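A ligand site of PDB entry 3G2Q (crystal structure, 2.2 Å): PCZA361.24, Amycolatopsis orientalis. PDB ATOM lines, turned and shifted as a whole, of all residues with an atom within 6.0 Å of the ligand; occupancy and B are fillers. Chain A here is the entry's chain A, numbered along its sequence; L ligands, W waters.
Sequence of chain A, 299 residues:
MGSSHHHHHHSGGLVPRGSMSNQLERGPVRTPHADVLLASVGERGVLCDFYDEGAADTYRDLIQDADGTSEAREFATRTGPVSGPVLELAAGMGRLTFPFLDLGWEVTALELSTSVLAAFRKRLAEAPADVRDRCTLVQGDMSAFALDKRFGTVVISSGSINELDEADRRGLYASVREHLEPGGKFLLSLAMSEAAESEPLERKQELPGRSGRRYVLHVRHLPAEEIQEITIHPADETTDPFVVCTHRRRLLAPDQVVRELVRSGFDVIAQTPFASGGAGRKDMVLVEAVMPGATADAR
OE2 of Glu 111 is in hydrogen-bond range of O5 of the ligand (2.5 Å).
An oxygen (O1) of the ligand is in salt-bridge range of the guanidinium group (NE) of Arg 95 (2.6 Å).
A nitrogen (N6) of the ligand sits at hydrogen-bond distance from the backbone NH (N) of Met 142.
The side-chain carboxylate (OD1) of Asp 141 lies within hydrogen-bond range of a nitrogen (N5) of the ligand.
O of Ala 90 lies close to N1 of the ligand (3.4 Å).
N7 of the ligand lies within hydrogen-bond range of N of Leu 112 (3.5 Å).
The side-chain carboxylate (OE2) of Glu 88 is in salt-bridge range of a nitrogen (N1) of the ligand.
The backbone NH (N) of Gly 92 is in hydrogen-bond range of the side-chain carboxylate (OE1) of Glu 111 (2.9 Å).
The backbone NH of Gly 140 lies within hydrogen-bond range of the backbone carbonyl oxygen of Glu 111, at 2.9 Å.
OE2 of Glu 111 is in hydrogen-bond range of N of Ser 113, 3.1 Å away.
The guanidinium group (NH2) of Arg 95 lies within salt-bridge range of the side-chain carboxylate (OE1) of Glu 71 (3.0 Å).
The backbone NH (N) of Ala 90 sits at hydrogen-bond distance from the backbone carbonyl oxygen (O) of Leu 110, 2.8 Å away.
The side-chain hydroxyl of Ser 160 lies within hydrogen-bond range of the side-chain hydroxyl of Ser 157, at 3.2 Å.
N of Ala 91 is in hydrogen-bond range of O of Leu 110 (2.9 Å).
N of Leu 110 sits at hydrogen-bond distance from O of Glu 88, at 2.8 Å.
Merely in contact with the ligand: Gly 92 (3.4 Å), Gly 140 (3.4 Å), Glu 163 (3.5 Å), Ser 160 (3.5 Å), Ala 91 (3.5 Å), Ser 157 (3.8 Å), Gly 159 (3.8 Å), Leu 110 (3.9 Å) and Leu 164 (3.96 Å).
Hydrophobic or aromatic side chains within 4 Å of the ligand: Ala 90, Leu 110, Leu 112, Met 142 and Leu 164.
Of the 26 residues printed, 16 come within 4 Å of the ligand.
The nearest printed residue that does not touch the ligand is Ser 113 (4.02 Å).
Water W3 lies within hydrogen-bond range of OE2 of Glu 88, O of Ala 91, N of Leu 96 and N1 of the ligand.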
ATOM      1  N   ALA A  66      27.296  40.095 -10.620  1.00  0.00           N
ATOM      2  CA  ALA A  66      28.173  38.990 -11.004  1.00  0.00           C
ATOM      3  C   ALA A  66      28.664  39.135 -12.451  1.00  0.00           C
ATOM      4  O   ALA A  66      27.878  39.090 -13.411  1.00  0.00           O
ATOM      5  CB  ALA A  66      27.473  37.637 -10.795  1.00  0.00           C
ATOM      6  N   GLU A  71      37.623  36.200 -16.169  1.00  0.00           N
ATOM      7  CA  GLU A  71      37.924  34.818 -15.803  1.00  0.00           C
ATOM      8  C   GLU A  71      37.600  33.893 -16.981  1.00  0.00           C
ATOM      9  O   GLU A  71      38.420  33.067 -17.362  1.00  0.00           O
ATOM     10  CB  GLU A  71      37.175  34.390 -14.527  1.00  0.00           C
ATOM     11  CG  GLU A  71      37.608  33.021 -14.022  1.00  0.00           C
ATOM     12  CD  GLU A  71      36.925  32.565 -12.748  1.00  0.00           C
ATOM     13  OE1 GLU A  71      36.187  33.332 -12.104  1.00  0.00           O
ATOM     14  OE2 GLU A  71      37.134  31.400 -12.373  1.00  0.00           O
ATOM     15  N   GLU A  88      31.023  22.386 -18.248  1.00  0.00           N
ATOM     16  CA  GLU A  88      31.245  23.273 -17.102  1.00  0.00           C
ATOM     17  C   GLU A  88      30.585  22.784 -15.819  1.00  0.00           C
ATOM     18  O   GLU A  88      29.360  22.601 -15.765  1.00  0.00           O
ATOM     19  CB  GLU A  88      30.817  24.715 -17.406  1.00  0.00           C
ATOM     20  CG  GLU A  88      31.183  25.633 -16.258  1.00  0.00           C
ATOM     21  CD  GLU A  88      30.514  26.978 -16.314  1.00  0.00           C
ATOM     22  OE1 GLU A  88      29.713  27.236 -17.241  1.00  0.00           O
ATOM     23  OE2 GLU A  88      30.796  27.790 -15.416  1.00  0.00           O
ATOM     24  N   LEU A  89      31.413  22.599 -14.765  1.00  0.00           N
ATOM     25  CA  LEU A  89      30.958  22.014 -13.494  1.00  0.00           C
ATOM     26  C   LEU A  89      30.621  23.058 -12.477  1.00  0.00           C
ATOM     27  O   LEU A  89      31.362  24.056 -12.341  1.00  0.00           O
ATOM     28  CB  LEU A  89      32.040  21.070 -12.893  1.00  0.00           C
ATOM     29  CG  LEU A  89      32.504  19.956 -13.833  1.00  0.00           C
ATOM     30  CD1 LEU A  89      33.712  19.164 -13.244  1.00  0.00           C
ATOM     31  CD2 LEU A  89      31.333  19.030 -14.180  1.00  0.00           C
ATOM     32  N   ALA A  90      29.548  22.808 -11.727  1.00  0.00           N
ATOM     33  CA  ALA A  90      29.001  23.783 -10.780  1.00  0.00           C
ATOM     34  C   ALA A  90      28.771  25.154 -11.470  1.00  0.00           C
ATOM     35  O   ALA A  90      29.261  26.207 -11.012  1.00  0.00           O
ATOM     36  CB  ALA A  90      29.904  23.904  -9.582  1.00  0.00           C
ATOM     37  N   ALA A  91      28.013  25.128 -12.562  1.00  0.00           N
ATOM     38  CA  ALA A  91      27.876  26.314 -13.410  1.00  0.00           C
ATOM     39  C   ALA A  91      27.114  27.470 -12.745  1.00  0.00           C
ATOM     40  O   ALA A  91      27.185  28.631 -13.195  1.00  0.00           O
ATOM     41  CB  ALA A  91      27.255  25.942 -14.723  1.00  0.00           C
ATOM     42  N   GLY A  92      26.409  27.175 -11.656  1.00  0.00           N
ATOM     43  CA  GLY A  92      25.689  28.209 -10.925  1.00  0.00           C
ATOM     44  C   GLY A  92      24.609  28.783 -11.841  1.00  0.00           C
ATOM     45  O   GLY A  92      23.881  28.030 -12.499  1.00  0.00           O
ATOM     46  N   MET A  93      24.505  30.101 -11.887  1.00  0.00           N
ATOM     47  CA  MET A  93      23.527  30.714 -12.789  1.00  0.00           C
ATOM     48  C   MET A  93      24.114  31.233 -14.099  1.00  0.00           C
ATOM     49  O   MET A  93      23.482  32.029 -14.797  1.00  0.00           O
ATOM     50  CB  MET A  93      22.765  31.830 -12.063  1.00  0.00           C
ATOM     51  CG  MET A  93      21.992  31.368 -10.848  1.00  0.00           C
ATOM     52  SD  MET A  93      21.333  32.787 -10.008  1.00  0.00           S
ATOM     53  CE  MET A  93      20.826  33.775 -11.397  1.00  0.00           C
ATOM     54  N   GLY A  94      25.325  30.777 -14.430  1.00  0.00           N
ATOM     55  CA  GLY A  94      25.940  31.090 -15.714  1.00  0.00           C
ATOM     56  C   GLY A  94      26.852  32.300 -15.777  1.00  0.00           C
ATOM     57  O   GLY A  94      27.107  32.821 -16.874  1.00  0.00           O
ATOM     58  N   ARG A  95      27.350  32.756 -14.638  1.00  0.00           N
ATOM     59  CA  ARG A  95      28.353  33.848 -14.598  1.00  0.00           C
ATOM     60  C   ARG A  95      29.533  33.611 -15.556  1.00  0.00           C
ATOM     61  O   ARG A  95      30.033  34.562 -16.164  1.00  0.00           O
ATOM     62  CB  ARG A  95      28.847  34.097 -13.161  1.00  0.00           C
ATOM     63  CG  ARG A  95      29.922  35.192 -13.035  1.00  0.00           C
ATOM     64  CD  ARG A  95      30.420  35.412 -11.600  1.00  0.00           C
ATOM     65  NE  ARG A  95      31.363  34.370 -11.151  1.00  0.00           N
ATOM     66  CZ  ARG A  95      32.682  34.389 -11.355  1.00  0.00           C
ATOM     67  NH1 ARG A  95      33.263  35.389 -12.011  1.00  0.00           N
ATOM     68  NH2 ARG A  95      33.427  33.389 -10.915  1.00  0.00           N
ATOM     69  N   LEU A  96      29.974  32.376 -15.729  1.00  0.00           N
ATOM     70  CA  LEU A  96      30.989  32.081 -16.726  1.00  0.00           C
ATOM     71  C   LEU A  96      30.393  31.493 -17.985  1.00  0.00           C
ATOM     72  O   LEU A  96      30.921  31.682 -19.070  1.00  0.00           O
ATOM     73  CB  LEU A  96      32.073  31.127 -16.178  1.00  0.00           C
ATOM     74  CG  LEU A  96      33.028  31.574 -15.073  1.00  0.00           C
ATOM     75  CD1 LEU A  96      34.137  30.543 -14.912  1.00  0.00           C
ATOM     76  CD2 LEU A  96      33.611  32.947 -15.356  1.00  0.00           C
ATOM     77  N   LEU A 110      26.624  21.839 -15.670  1.00  0.00           N
ATOM     78  CA  LEU A 110      26.173  20.955 -14.622  1.00  0.00           C
ATOM     79  C   LEU A 110      26.072  21.706 -13.302  1.00  0.00           C
ATOM     80  O   LEU A 110      27.016  22.424 -12.907  1.00  0.00           O
ATOM     81  CB  LEU A 110      27.130  19.753 -14.509  1.00  0.00           C
ATOM     82  CG  LEU A 110      26.812  18.712 -13.431  1.00  0.00           C
ATOM     83  CD1 LEU A 110      27.139  17.320 -13.894  1.00  0.00           C
ATOM     84  CD2 LEU A 110      27.589  19.055 -12.149  1.00  0.00           C
ATOM     85  N   GLU A 111      24.967  21.527 -12.599  1.00  0.00           N
ATOM     86  CA  GLU A 111      24.769  22.238 -11.374  1.00  0.00           C
ATOM     87  C   GLU A 111      23.923  21.340 -10.473  1.00  0.00           C
ATOM     88  O   GLU A 111      23.120  20.547 -10.983  1.00  0.00           O
ATOM     89  CB  GLU A 111      24.082  23.614 -11.677  1.00  0.00           C
ATOM     90  CG  GLU A 111      23.452  24.328 -10.505  1.00  0.00           C
ATOM     91  CD  GLU A 111      24.442  24.694  -9.406  1.00  0.00           C
ATOM     92  OE1 GLU A 111      25.557  25.140  -9.731  1.00  0.00           O
ATOM     93  OE2 GLU A 111      24.082  24.567  -8.206  1.00  0.00           O
ATOM     94  N   LEU A 112      24.148  21.438  -9.158  1.00  0.00           N
ATOM     95  CA  LEU A 112      23.472  20.589  -8.160  1.00  0.00           C
ATOM     96  C   LEU A 112      22.119  21.116  -7.663  1.00  0.00           C
ATOM     97  O   LEU A 112      21.159  20.342  -7.495  1.00  0.00           O
ATOM     98  CB  LEU A 112      24.389  20.331  -6.944  1.00  0.00           C
ATOM     99  CG  LEU A 112      23.946  19.338  -5.840  1.00  0.00           C
ATOM    100  CD1 LEU A 112      23.550  18.027  -6.421  1.00  0.00           C
ATOM    101  CD2 LEU A 112      25.014  19.137  -4.764  1.00  0.00           C
ATOM    102  N   SER A 113      22.039  22.415  -7.397  1.00  0.00           N
ATOM    103  CA  SER A 113      20.846  23.005  -6.814  1.00  0.00           C
ATOM    104  C   SER A 113      19.758  23.230  -7.860  1.00  0.00           C
ATOM    105  O   SER A 113      19.997  23.819  -8.929  1.00  0.00           O
ATOM    106  CB  SER A 113      21.179  24.322  -6.112  1.00  0.00           C
ATOM    107  OG  SER A 113      20.080  25.190  -6.175  1.00  0.00           O
ATOM    108  N   VAL A 116      18.871  27.010  -8.282  1.00  0.00           N
ATOM    109  CA  VAL A 116      19.881  27.659  -9.131  1.00  0.00           C
ATOM    110  C   VAL A 116      19.695  27.307 -10.609  1.00  0.00           C
ATOM    111  O   VAL A 116      19.812  28.188 -11.467  1.00  0.00           O
ATOM    112  CB  VAL A 116      21.329  27.358  -8.628  1.00  0.00           C
ATOM    113  CG1 VAL A 116      22.372  27.912  -9.593  1.00  0.00           C
ATOM    114  CG2 VAL A 116      21.547  27.935  -7.244  1.00  0.00           C
ATOM    115  N   GLY A 140      23.316  17.672 -11.476  1.00  0.00           N
ATOM    116  CA  GLY A 140      24.244  16.650 -11.026  1.00  0.00           C
ATOM    117  C   GLY A 140      25.193  17.121  -9.960  1.00  0.00           C
ATOM    118  O   GLY A 140      25.347  18.323  -9.752  1.00  0.00           O
ATOM    119  N   ASP A 141      25.812  16.155  -9.303  1.00  0.00           N
ATOM    120  CA  ASP A 141      26.797  16.352  -8.251  1.00  0.00           C
ATOM    121  C   ASP A 141      28.173  16.280  -8.890  1.00  0.00           C
ATOM    122  O   ASP A 141      28.547  15.230  -9.363  1.00  0.00           O
ATOM    123  CB  ASP A 141      26.669  15.202  -7.228  1.00  0.00           C
ATOM    124  CG  ASP A 141      27.453  15.453  -5.958  1.00  0.00           C
ATOM    125  OD1 ASP A 141      28.533  16.104  -6.001  1.00  0.00           O
ATOM    126  OD2 ASP A 141      26.987  14.981  -4.904  1.00  0.00           O
ATOM    127  N   MET A 142      28.929  17.376  -8.903  1.00  0.00           N
ATOM    128  CA  MET A 142      30.229  17.365  -9.618  1.00  0.00           C
ATOM    129  C   MET A 142      31.270  16.410  -8.937  1.00  0.00           C
ATOM    130  O   MET A 142      32.323  16.105  -9.529  1.00  0.00           O
ATOM    131  CB  MET A 142      30.800  18.752  -9.721  1.00  0.00           C
ATOM    132  CG  MET A 142      31.129  19.336  -8.353  1.00  0.00           C
ATOM    133  SD  MET A 142      31.872  20.940  -8.405  1.00  0.00           S
ATOM    134  CE  MET A 142      31.413  21.594  -6.808  1.00  0.00           C
ATOM    135  N   SER A 143      30.956  15.925  -7.739  1.00  0.00           N
ATOM    136  CA  SER A 143      31.804  14.934  -7.061  1.00  0.00           C
ATOM    137  C   SER A 143      31.517  13.473  -7.466  1.00  0.00           C
ATOM    138  O   SER A 143      32.357  12.600  -7.248  1.00  0.00           O
ATOM    139  CB  SER A 143      31.748  15.134  -5.542  1.00  0.00           C
ATOM    140  OG  SER A 143      30.613  14.552  -4.943  1.00  0.00           O
ATOM    141  N   SER A 157      35.376  26.522 -11.699  1.00  0.00           N
ATOM    142  CA  SER A 157      35.951  27.706 -11.052  1.00  0.00           C
ATOM    143  C   SER A 157      36.275  27.539  -9.570  1.00  0.00           C
ATOM    144  O   SER A 157      35.716  26.662  -8.887  1.00  0.00           O
ATOM    145  CB  SER A 157      35.088  28.919 -11.257  1.00  0.00           C
ATOM    146  OG  SER A 157      33.895  28.726 -10.510  1.00  0.00           O
ATOM    147  N   GLY A 159      35.426  29.185  -6.902  1.00  0.00           N
ATOM    148  CA  GLY A 159      34.264  29.236  -6.016  1.00  0.00           C
ATOM    149  C   GLY A 159      33.751  27.832  -5.781  1.00  0.00           C
ATOM    150  O   GLY A 159      33.277  27.498  -4.671  1.00  0.00           O
ATOM    151  N   SER A 160      33.915  27.013  -6.834  1.00  0.00           N
ATOM    152  CA  SER A 160      33.269  25.717  -6.939  1.00  0.00           C
ATOM    153  C   SER A 160      34.097  24.560  -6.366  1.00  0.00           C
ATOM    154  O   SER A 160      33.578  23.786  -5.565  1.00  0.00           O
ATOM    155  CB  SER A 160      32.933  25.460  -8.400  1.00  0.00           C
ATOM    156  OG  SER A 160      32.214  26.559  -8.885  1.00  0.00           O
ATOM    157  N   GLU A 163      34.082  24.292  -2.802  1.00  0.00           N
ATOM    158  CA  GLU A 163      32.845  23.745  -2.271  1.00  0.00           C
ATOM    159  C   GLU A 163      33.053  22.331  -1.711  1.00  0.00           C
ATOM    160  O   GLU A 163      32.282  21.883  -0.894  1.00  0.00           O
ATOM    161  CB  GLU A 163      31.784  23.643  -3.392  1.00  0.00           C
ATOM    162  CG  GLU A 163      31.303  24.998  -3.968  1.00  0.00           C
ATOM    163  CD  GLU A 163      30.439  25.773  -3.029  1.00  0.00           C
ATOM    164  OE1 GLU A 163      29.468  25.200  -2.494  1.00  0.00           O
ATOM    165  OE2 GLU A 163      30.729  26.970  -2.822  1.00  0.00           O
ATOM    166  N   LEU A 164      34.091  21.643  -2.168  1.00  0.00           N
ATOM    167  CA  LEU A 164      34.240  20.198  -1.877  1.00  0.00           C
ATOM    168  C   LEU A 164      35.281  19.882  -0.832  1.00  0.00           C
ATOM    169  O   LEU A 164      36.398  20.423  -0.883  1.00  0.00           O
ATOM    170  CB  LEU A 164      34.573  19.466  -3.178  1.00  0.00           C
ATOM    171  CG  LEU A 164      33.542  19.561  -4.314  1.00  0.00           C
ATOM    172  CD1 LEU A 164      34.054  18.770  -5.498  1.00  0.00           C
ATOM    173  CD2 LEU A 164      32.171  19.008  -3.819  1.00  0.00           C
ATOM    174  N   ARG A 249      34.572  30.489   4.330  1.00  0.00           N
ATOM    175  CA  ARG A 249      34.648  29.427   3.323  1.00  0.00           C
ATOM    176  C   ARG A 249      36.051  28.829   3.197  1.00  0.00           C
ATOM    177  O   ARG A 249      37.047  29.454   3.574  1.00  0.00           O
ATOM    178  CB  ARG A 249      34.046  29.852   1.963  1.00  0.00           C
ATOM    179  CG  ARG A 249      34.671  31.045   1.274  1.00  0.00           C
ATOM    180  CD  ARG A 249      34.058  31.251  -0.137  1.00  0.00           C
ATOM    181  NE  ARG A 249      34.415  32.549  -0.744  1.00  0.00           N
ATOM    182  CZ  ARG A 249      34.106  32.916  -1.998  1.00  0.00           C
ATOM    183  NH1 ARG A 249      33.424  32.101  -2.799  1.00  0.00           N
ATOM    184  NH2 ARG A 249      34.490  34.106  -2.451  1.00  0.00           N
HETATM  185  N1  LIG L   1      30.387  29.286 -11.821  1.00  0.00           N
HETATM  186  C1  LIG L   1      29.541  29.845 -10.730  1.00  0.00           C
HETATM  187  C2  LIG L   1      29.822  31.310 -10.596  1.00  0.00           C
HETATM  188  O1  LIG L   1      30.914  31.776 -10.931  1.00  0.00           O
HETATM  189  O2  LIG L   1      28.952  32.069 -10.145  1.00  0.00           O
HETATM  190  C3  LIG L   1      29.821  29.121  -9.409  1.00  0.00           C
HETATM  191  C4  LIG L   1      28.848  29.506  -8.296  1.00  0.00           C
HETATM  192  C5  LIG L   1      29.286  29.142  -6.856  1.00  0.00           C
HETATM  193  N2  LIG L   1      30.521  29.841  -6.526  1.00  0.00           N
HETATM  194  C6  LIG L   1      29.438  27.634  -6.575  1.00  0.00           C
HETATM  195  C7  LIG L   1      28.306  26.739  -7.104  1.00  0.00           C
HETATM  196  O3  LIG L   1      28.564  25.354  -6.872  1.00  0.00           O
HETATM  197  C8  LIG L   1      26.911  26.986  -6.540  1.00  0.00           C
HETATM  198  O4  LIG L   1      26.124  27.253  -7.692  1.00  0.00           O
HETATM  199  C9  LIG L   1      26.462  25.668  -5.911  1.00  0.00           C
HETATM  200  O5  LIG L   1      25.062  25.379  -6.063  1.00  0.00           O
HETATM  201  C10 LIG L   1      27.299  24.696  -6.725  1.00  0.00           C
HETATM  202  N3  LIG L   1      27.605  23.383  -6.123  1.00  0.00           N
HETATM  203  C11 LIG L   1      27.953  23.141  -4.855  1.00  0.00           C
HETATM  204  N4  LIG L   1      28.239  21.827  -4.669  1.00  0.00           N
HETATM  205  C12 LIG L   1      28.059  21.219  -5.847  1.00  0.00           C
HETATM  206  C13 LIG L   1      28.197  19.836  -6.351  1.00  0.00           C
HETATM  207  N5  LIG L   1      28.584  18.835  -5.489  1.00  0.00           N
HETATM  208  N6  LIG L   1      27.946  19.644  -7.690  1.00  0.00           N
HETATM  209  C14 LIG L   1      27.582  20.626  -8.542  1.00  0.00           C
HETATM  210  N7  LIG L   1      27.440  21.915  -8.138  1.00  0.00           N
HETATM  211  C15 LIG L   1      27.667  22.249  -6.834  1.00  0.00           C
HETATM  212  O   HOH W   1      31.902  32.323  -6.635  1.00  0.00           O
HETATM  213  O   HOH W   2      25.064  30.006  -7.302  1.00  0.00           O
HETATM  214  O   HOH W   3      29.173  29.729 -14.634  1.00  0.00           O
HETATM  215  O   HOH W   4      26.753  31.843 -11.497  1.00  0.00           O
